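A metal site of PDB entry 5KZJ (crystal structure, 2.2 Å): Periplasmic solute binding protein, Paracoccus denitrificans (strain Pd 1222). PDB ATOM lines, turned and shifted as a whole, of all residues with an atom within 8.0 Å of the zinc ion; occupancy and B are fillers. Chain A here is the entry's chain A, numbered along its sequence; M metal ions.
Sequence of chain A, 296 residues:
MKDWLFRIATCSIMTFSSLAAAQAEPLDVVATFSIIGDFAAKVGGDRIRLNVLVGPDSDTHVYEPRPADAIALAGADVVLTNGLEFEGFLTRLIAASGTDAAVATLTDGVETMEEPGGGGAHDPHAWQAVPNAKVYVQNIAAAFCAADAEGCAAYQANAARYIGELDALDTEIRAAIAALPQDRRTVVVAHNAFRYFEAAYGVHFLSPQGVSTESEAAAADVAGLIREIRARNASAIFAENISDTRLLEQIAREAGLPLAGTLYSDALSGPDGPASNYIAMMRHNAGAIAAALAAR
The zinc ion is bound by a ring nitrogen (NE2) of His 125 (2.0 Å), a ring nitrogen (NE2) of His 61 (2.0 Å), a ring nitrogen (NE2) of His 191 (2.0 Å) and the side-chain carboxylate of Asp 266 (2.2 Å).
The zinc ion has four donor atoms within binding distance.
Val 211 touches the zinc ion.
A ring nitrogen (ND1) of His 191 lies within hydrogen-bond range of the side-chain carboxylate of Glu 240 (2.8 Å).
NE2 of His 61 sits close to O of Val 211 (3.4 Å).
The side-chain carboxylate (OD1) of Asp 123 lies within hydrogen-bond range of a ring nitrogen (ND1) of His 125 (2.7 Å).
OD1 of Asp 59 is in hydrogen-bond range of N of His 61.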
ATOM      1  N   ASP A  59     -27.264  12.489   3.580  1.00  0.00           N
ATOM      2  CA  ASP A  59     -25.956  12.397   4.243  1.00  0.00           C
ATOM      3  C   ASP A  59     -24.827  12.562   3.219  1.00  0.00           C
ATOM      4  O   ASP A  59     -24.632  11.785   2.324  1.00  0.00           O
ATOM      5  CB  ASP A  59     -25.853  11.076   5.012  1.00  0.00           C
ATOM      6  CG  ASP A  59     -24.451  10.779   5.541  1.00  0.00           C
ATOM      7  OD1 ASP A  59     -23.487  11.584   5.389  1.00  0.00           O
ATOM      8  OD2 ASP A  59     -24.306   9.729   6.196  1.00  0.00           O
ATOM      9  N   THR A  60     -24.051  13.632   3.419  1.00  0.00           N
ATOM     10  CA  THR A  60     -23.069  14.093   2.484  1.00  0.00           C
ATOM     11  C   THR A  60     -21.819  13.215   2.588  1.00  0.00           C
ATOM     12  O   THR A  60     -21.050  13.115   1.615  1.00  0.00           O
ATOM     13  CB  THR A  60     -22.808  15.620   2.766  1.00  0.00           C
ATOM     14  OG1 THR A  60     -23.975  16.399   2.489  1.00  0.00           O
ATOM     15  CG2 THR A  60     -21.740  16.206   1.952  1.00  0.00           C
ATOM     16  N   HIS A  61     -21.594  12.599   3.748  1.00  0.00           N
ATOM     17  CA  HIS A  61     -20.374  11.851   3.956  1.00  0.00           C
ATOM     18  C   HIS A  61     -20.343  10.682   2.994  1.00  0.00           C
ATOM     19  O   HIS A  61     -19.303  10.306   2.543  1.00  0.00           O
ATOM     20  CB  HIS A  61     -20.282  11.296   5.371  1.00  0.00           C
ATOM     21  CG  HIS A  61     -20.165  12.316   6.446  1.00  0.00           C
ATOM     22  ND1 HIS A  61     -19.043  13.103   6.624  1.00  0.00           N
ATOM     23  CD2 HIS A  61     -20.998  12.622   7.472  1.00  0.00           C
ATOM     24  CE1 HIS A  61     -19.193  13.847   7.704  1.00  0.00           C
ATOM     25  NE2 HIS A  61     -20.377  13.593   8.231  1.00  0.00           N
ATOM     26  N   PHE A  86     -15.490  17.647   3.727  1.00  0.00           N
ATOM     27  CA  PHE A  86     -16.833  17.185   3.928  1.00  0.00           C
ATOM     28  C   PHE A  86     -17.366  16.463   2.668  1.00  0.00           C
ATOM     29  O   PHE A  86     -17.913  15.336   2.727  1.00  0.00           O
ATOM     30  CB  PHE A  86     -17.694  18.389   4.275  1.00  0.00           C
ATOM     31  CG  PHE A  86     -19.052  18.031   4.698  1.00  0.00           C
ATOM     32  CD1 PHE A  86     -19.246  17.104   5.695  1.00  0.00           C
ATOM     33  CD2 PHE A  86     -20.159  18.650   4.106  1.00  0.00           C
ATOM     34  CE1 PHE A  86     -20.518  16.795   6.116  1.00  0.00           C
ATOM     35  CE2 PHE A  86     -21.430  18.314   4.481  1.00  0.00           C
ATOM     36  CZ  PHE A  86     -21.616  17.385   5.485  1.00  0.00           C
ATOM     37  N   ASP A 123     -12.283  18.583  11.376  1.00  0.00           N
ATOM     38  CA  ASP A 123     -13.732  18.275  11.536  1.00  0.00           C
ATOM     39  C   ASP A 123     -14.506  19.270  10.706  1.00  0.00           C
ATOM     40  O   ASP A 123     -14.340  20.492  10.887  1.00  0.00           O
ATOM     41  CB  ASP A 123     -14.040  18.429  13.012  1.00  0.00           C
ATOM     42  CG  ASP A 123     -15.442  18.121  13.361  1.00  0.00           C
ATOM     43  OD1 ASP A 123     -16.369  18.126  12.461  1.00  0.00           O
ATOM     44  OD2 ASP A 123     -15.603  17.939  14.578  1.00  0.00           O
ATOM     45  N   PRO A 124     -15.274  18.799   9.717  1.00  0.00           N
ATOM     46  CA  PRO A 124     -15.926  19.723   8.779  1.00  0.00           C
ATOM     47  C   PRO A 124     -17.194  20.397   9.337  1.00  0.00           C
ATOM     48  O   PRO A 124     -17.769  21.255   8.671  1.00  0.00           O
ATOM     49  CB  PRO A 124     -16.396  18.784   7.656  1.00  0.00           C
ATOM     50  CG  PRO A 124     -16.680  17.476   8.399  1.00  0.00           C
ATOM     51  CD  PRO A 124     -15.585  17.377   9.416  1.00  0.00           C
ATOM     52  N   HIS A 125     -17.666  19.970  10.509  1.00  0.00           N
ATOM     53  CA  HIS A 125     -18.993  20.369  10.992  1.00  0.00           C
ATOM     54  C   HIS A 125     -19.011  21.758  11.627  1.00  0.00           C
ATOM     55  O   HIS A 125     -19.557  21.945  12.685  1.00  0.00           O
ATOM     56  CB  HIS A 125     -19.531  19.348  11.986  1.00  0.00           C
ATOM     57  CG  HIS A 125     -19.644  17.957  11.443  1.00  0.00           C
ATOM     58  ND1 HIS A 125     -18.679  16.987  11.667  1.00  0.00           N
ATOM     59  CD2 HIS A 125     -20.621  17.351  10.742  1.00  0.00           C
ATOM     60  CE1 HIS A 125     -19.067  15.844  11.130  1.00  0.00           C
ATOM     61  NE2 HIS A 125     -20.208  16.052  10.500  1.00  0.00           N
ATOM     62  N   TRP A 127     -20.552  24.559  11.026  1.00  0.00           N
ATOM     63  CA  TRP A 127     -21.809  25.314  11.126  1.00  0.00           C
ATOM     64  C   TRP A 127     -22.605  25.097  12.423  1.00  0.00           C
ATOM     65  O   TRP A 127     -23.602  25.776  12.695  1.00  0.00           O
ATOM     66  CB  TRP A 127     -22.722  24.902   9.978  1.00  0.00           C
ATOM     67  CG  TRP A 127     -23.073  23.451   9.994  1.00  0.00           C
ATOM     68  CD1 TRP A 127     -24.029  22.892  10.725  1.00  0.00           C
ATOM     69  CD2 TRP A 127     -22.444  22.392   9.283  1.00  0.00           C
ATOM     70  NE1 TRP A 127     -24.074  21.549  10.523  1.00  0.00           N
ATOM     71  CE2 TRP A 127     -23.098  21.208   9.648  1.00  0.00           C
ATOM     72  CE3 TRP A 127     -21.385  22.313   8.404  1.00  0.00           C
ATOM     73  CZ2 TRP A 127     -22.736  19.974   9.149  1.00  0.00           C
ATOM     74  CZ3 TRP A 127     -21.052  21.094   7.880  1.00  0.00           C
ATOM     75  CH2 TRP A 127     -21.691  19.934   8.276  1.00  0.00           C
ATOM     76  N   HIS A 191     -23.653  10.446  15.431  1.00  0.00           N
ATOM     77  CA  HIS A 191     -22.268  10.519  14.948  1.00  0.00           C
ATOM     78  C   HIS A 191     -21.635  11.704  15.556  1.00  0.00           C
ATOM     79  O   HIS A 191     -22.274  12.503  16.178  1.00  0.00           O
ATOM     80  CB  HIS A 191     -22.080  10.360  13.390  1.00  0.00           C
ATOM     81  CG  HIS A 191     -22.259  11.600  12.566  1.00  0.00           C
ATOM     82  ND1 HIS A 191     -23.525  12.093  12.261  1.00  0.00           N
ATOM     83  CD2 HIS A 191     -21.396  12.311  11.809  1.00  0.00           C
ATOM     84  CE1 HIS A 191     -23.423  13.120  11.459  1.00  0.00           C
ATOM     85  NE2 HIS A 191     -22.158  13.243  11.108  1.00  0.00           N
ATOM     86  N   ASN A 192     -20.333  11.787  15.410  1.00  0.00           N
ATOM     87  CA  ASN A 192     -19.607  12.777  16.105  1.00  0.00           C
ATOM     88  C   ASN A 192     -19.597  14.111  15.330  1.00  0.00           C
ATOM     89  O   ASN A 192     -18.560  14.558  14.751  1.00  0.00           O
ATOM     90  CB  ASN A 192     -18.191  12.240  16.402  1.00  0.00           C
ATOM     91  CG  ASN A 192     -17.524  12.968  17.528  1.00  0.00           C
ATOM     92  OD1 ASN A 192     -18.053  13.981  18.018  1.00  0.00           O
ATOM     93  ND2 ASN A 192     -16.357  12.477  17.964  1.00  0.00           N
ATOM     94  N   ALA A 193     -20.761  14.763  15.368  1.00  0.00           N
ATOM     95  CA  ALA A 193     -21.094  15.891  14.447  1.00  0.00           C
ATOM     96  C   ALA A 193     -21.315  17.256  15.139  1.00  0.00           C
ATOM     97  O   ALA A 193     -21.419  18.285  14.471  1.00  0.00           O
ATOM     98  CB  ALA A 193     -22.310  15.532  13.611  1.00  0.00           C
ATOM     99  N   PHE A 194     -21.266  17.276  16.473  1.00  0.00           N
ATOM    100  CA  PHE A 194     -21.520  18.465  17.193  1.00  0.00           C
ATOM    101  C   PHE A 194     -20.362  19.015  18.033  1.00  0.00           C
ATOM    102  O   PHE A 194     -20.577  19.786  18.999  1.00  0.00           O
ATOM    103  CB  PHE A 194     -22.712  18.163  18.115  1.00  0.00           C
ATOM    104  CG  PHE A 194     -23.931  17.781  17.413  1.00  0.00           C
ATOM    105  CD1 PHE A 194     -24.146  16.460  17.083  1.00  0.00           C
ATOM    106  CD2 PHE A 194     -24.918  18.729  17.082  1.00  0.00           C
ATOM    107  CE1 PHE A 194     -25.297  16.079  16.415  1.00  0.00           C
ATOM    108  CE2 PHE A 194     -26.082  18.342  16.426  1.00  0.00           C
ATOM    109  CZ  PHE A 194     -26.255  17.037  16.074  1.00  0.00           C
ATOM    110  N   GLY A 210     -18.047   7.983  14.523  1.00  0.00           N
ATOM    111  CA  GLY A 210     -17.115   9.060  14.501  1.00  0.00           C
ATOM    112  C   GLY A 210     -17.609  10.224  13.638  1.00  0.00           C
ATOM    113  O   GLY A 210     -18.827  10.399  13.412  1.00  0.00           O
ATOM    114  N   VAL A 211     -16.638  11.018  13.205  1.00  0.00           N
ATOM    115  CA  VAL A 211     -16.824  12.262  12.525  1.00  0.00           C
ATOM    116  C   VAL A 211     -17.509  12.066  11.207  1.00  0.00           C
ATOM    117  O   VAL A 211     -18.323  12.903  10.823  1.00  0.00           O
ATOM    118  CB  VAL A 211     -15.497  13.053  12.354  1.00  0.00           C
ATOM    119  CG1 VAL A 211     -15.762  14.388  11.680  1.00  0.00           C
ATOM    120  CG2 VAL A 211     -14.948  13.358  13.719  1.00  0.00           C
ATOM    121  N   SER A 212     -17.213  10.937  10.555  1.00  0.00           N
ATOM    122  CA  SER A 212     -17.902  10.527   9.395  1.00  0.00           C
ATOM    123  C   SER A 212     -18.749   9.314   9.644  1.00  0.00           C
ATOM    124  O   SER A 212     -18.427   8.508  10.466  1.00  0.00           O
ATOM    125  CB  SER A 212     -16.925  10.297   8.251  1.00  0.00           C
ATOM    126  OG  SER A 212     -17.631   9.813   7.080  1.00  0.00           O
ATOM    127  N   THR A 213     -19.857   9.222   8.905  1.00  0.00           N
ATOM    128  CA  THR A 213     -20.772   8.105   8.959  1.00  0.00           C
ATOM    129  C   THR A 213     -20.334   7.079   7.951  1.00  0.00           C
ATOM    130  O   THR A 213     -21.017   6.097   7.762  1.00  0.00           O
ATOM    131  CB  THR A 213     -22.197   8.514   8.498  1.00  0.00           C
ATOM    132  OG1 THR A 213     -22.087   9.277   7.276  1.00  0.00           O
ATOM    133  CG2 THR A 213     -22.884   9.348   9.563  1.00  0.00           C
ATOM    134  N   GLU A 214     -19.187   7.258   7.307  1.00  0.00           N
ATOM    135  CA  GLU A 214     -18.699   6.244   6.351  1.00  0.00           C
ATOM    136  C   GLU A 214     -18.601   4.831   6.947  1.00  0.00           C
ATOM    137  O   GLU A 214     -18.989   3.872   6.277  1.00  0.00           O
ATOM    138  CB  GLU A 214     -17.349   6.647   5.726  1.00  0.00           C
ATOM    139  CG  GLU A 214     -17.468   7.311   4.355  1.00  0.00           C
ATOM    140  CD  GLU A 214     -16.419   8.384   4.090  1.00  0.00           C
ATOM    141  OE1 GLU A 214     -15.887   8.432   2.962  1.00  0.00           O
ATOM    142  OE2 GLU A 214     -16.143   9.224   4.990  1.00  0.00           O
ATOM    143  N   GLU A 240     -30.727  11.088  14.719  1.00  0.00           N
ATOM    144  CA  GLU A 240     -30.387  12.153  13.776  1.00  0.00           C
ATOM    145  C   GLU A 240     -31.196  11.919  12.537  1.00  0.00           C
ATOM    146  O   GLU A 240     -31.413  10.749  12.140  1.00  0.00           O
ATOM    147  CB  GLU A 240     -28.894  12.178  13.364  1.00  0.00           C
ATOM    148  CG  GLU A 240     -28.034  12.855  14.428  1.00  0.00           C
ATOM    149  CD  GLU A 240     -26.534  12.691  14.168  1.00  0.00           C
ATOM    150  OE1 GLU A 240     -26.133  12.658  12.955  1.00  0.00           O
ATOM    151  OE2 GLU A 240     -25.780  12.592  15.156  1.00  0.00           O
ATOM    152  N   ILE A 242     -30.400  12.266   9.451  1.00  0.00           N
ATOM    153  CA  ILE A 242     -29.676  11.668   8.311  1.00  0.00           C
ATOM    154  C   ILE A 242     -29.482  10.152   8.434  1.00  0.00           C
ATOM    155  O   ILE A 242     -28.980   9.545   7.521  1.00  0.00           O
ATOM    156  CB  ILE A 242     -28.285  12.331   8.114  1.00  0.00           C
ATOM    157  CG1 ILE A 242     -27.396  12.169   9.363  1.00  0.00           C
ATOM    158  CG2 ILE A 242     -28.454  13.800   7.729  1.00  0.00           C
ATOM    159  CD1 ILE A 242     -25.941  12.476   9.143  1.00  0.00           C
ATOM    160  N   SER A 265     -28.358  17.133  12.227  1.00  0.00           N
ATOM    161  CA  SER A 265     -26.944  17.263  12.192  1.00  0.00           C
ATOM    162  C   SER A 265     -26.382  17.889  10.890  1.00  0.00           C
ATOM    163  O   SER A 265     -25.888  18.992  10.903  1.00  0.00           O
ATOM    164  CB  SER A 265     -26.298  15.921  12.492  1.00  0.00           C
ATOM    165  OG  SER A 265     -26.690  14.920  11.561  1.00  0.00           O
ATOM    166  N   ASP A 266     -26.390  17.155   9.791  1.00  0.00           N
ATOM    167  CA  ASP A 266     -25.722  17.602   8.568  1.00  0.00           C
ATOM    168  C   ASP A 266     -26.688  17.948   7.461  1.00  0.00           C
ATOM    169  O   ASP A 266     -26.273  18.126   6.298  1.00  0.00           O
ATOM    170  CB  ASP A 266     -24.831  16.495   8.046  1.00  0.00           C
ATOM    171  CG  ASP A 266     -23.713  16.119   9.036  1.00  0.00           C
ATOM    172  OD1 ASP A 266     -23.595  16.748  10.126  1.00  0.00           O
ATOM    173  OD2 ASP A 266     -22.939  15.276   8.653  1.00  0.00           O
ATOM    174  N   ALA A 267     -27.975  17.988   7.792  1.00  0.00           N
ATOM    175  CA  ALA A 267     -28.984  18.408   6.792  1.00  0.00           C
ATOM    176  C   ALA A 267     -30.183  19.041   7.444  1.00  0.00           C
ATOM    177  O   ALA A 267     -30.536  18.676   8.560  1.00  0.00           O
ATOM    178  CB  ALA A 267     -29.444  17.223   5.960  1.00  0.00           C
HETATM  179 ZN    ZN M   1     -21.243  14.529   9.818  1.00  0.00          ZN
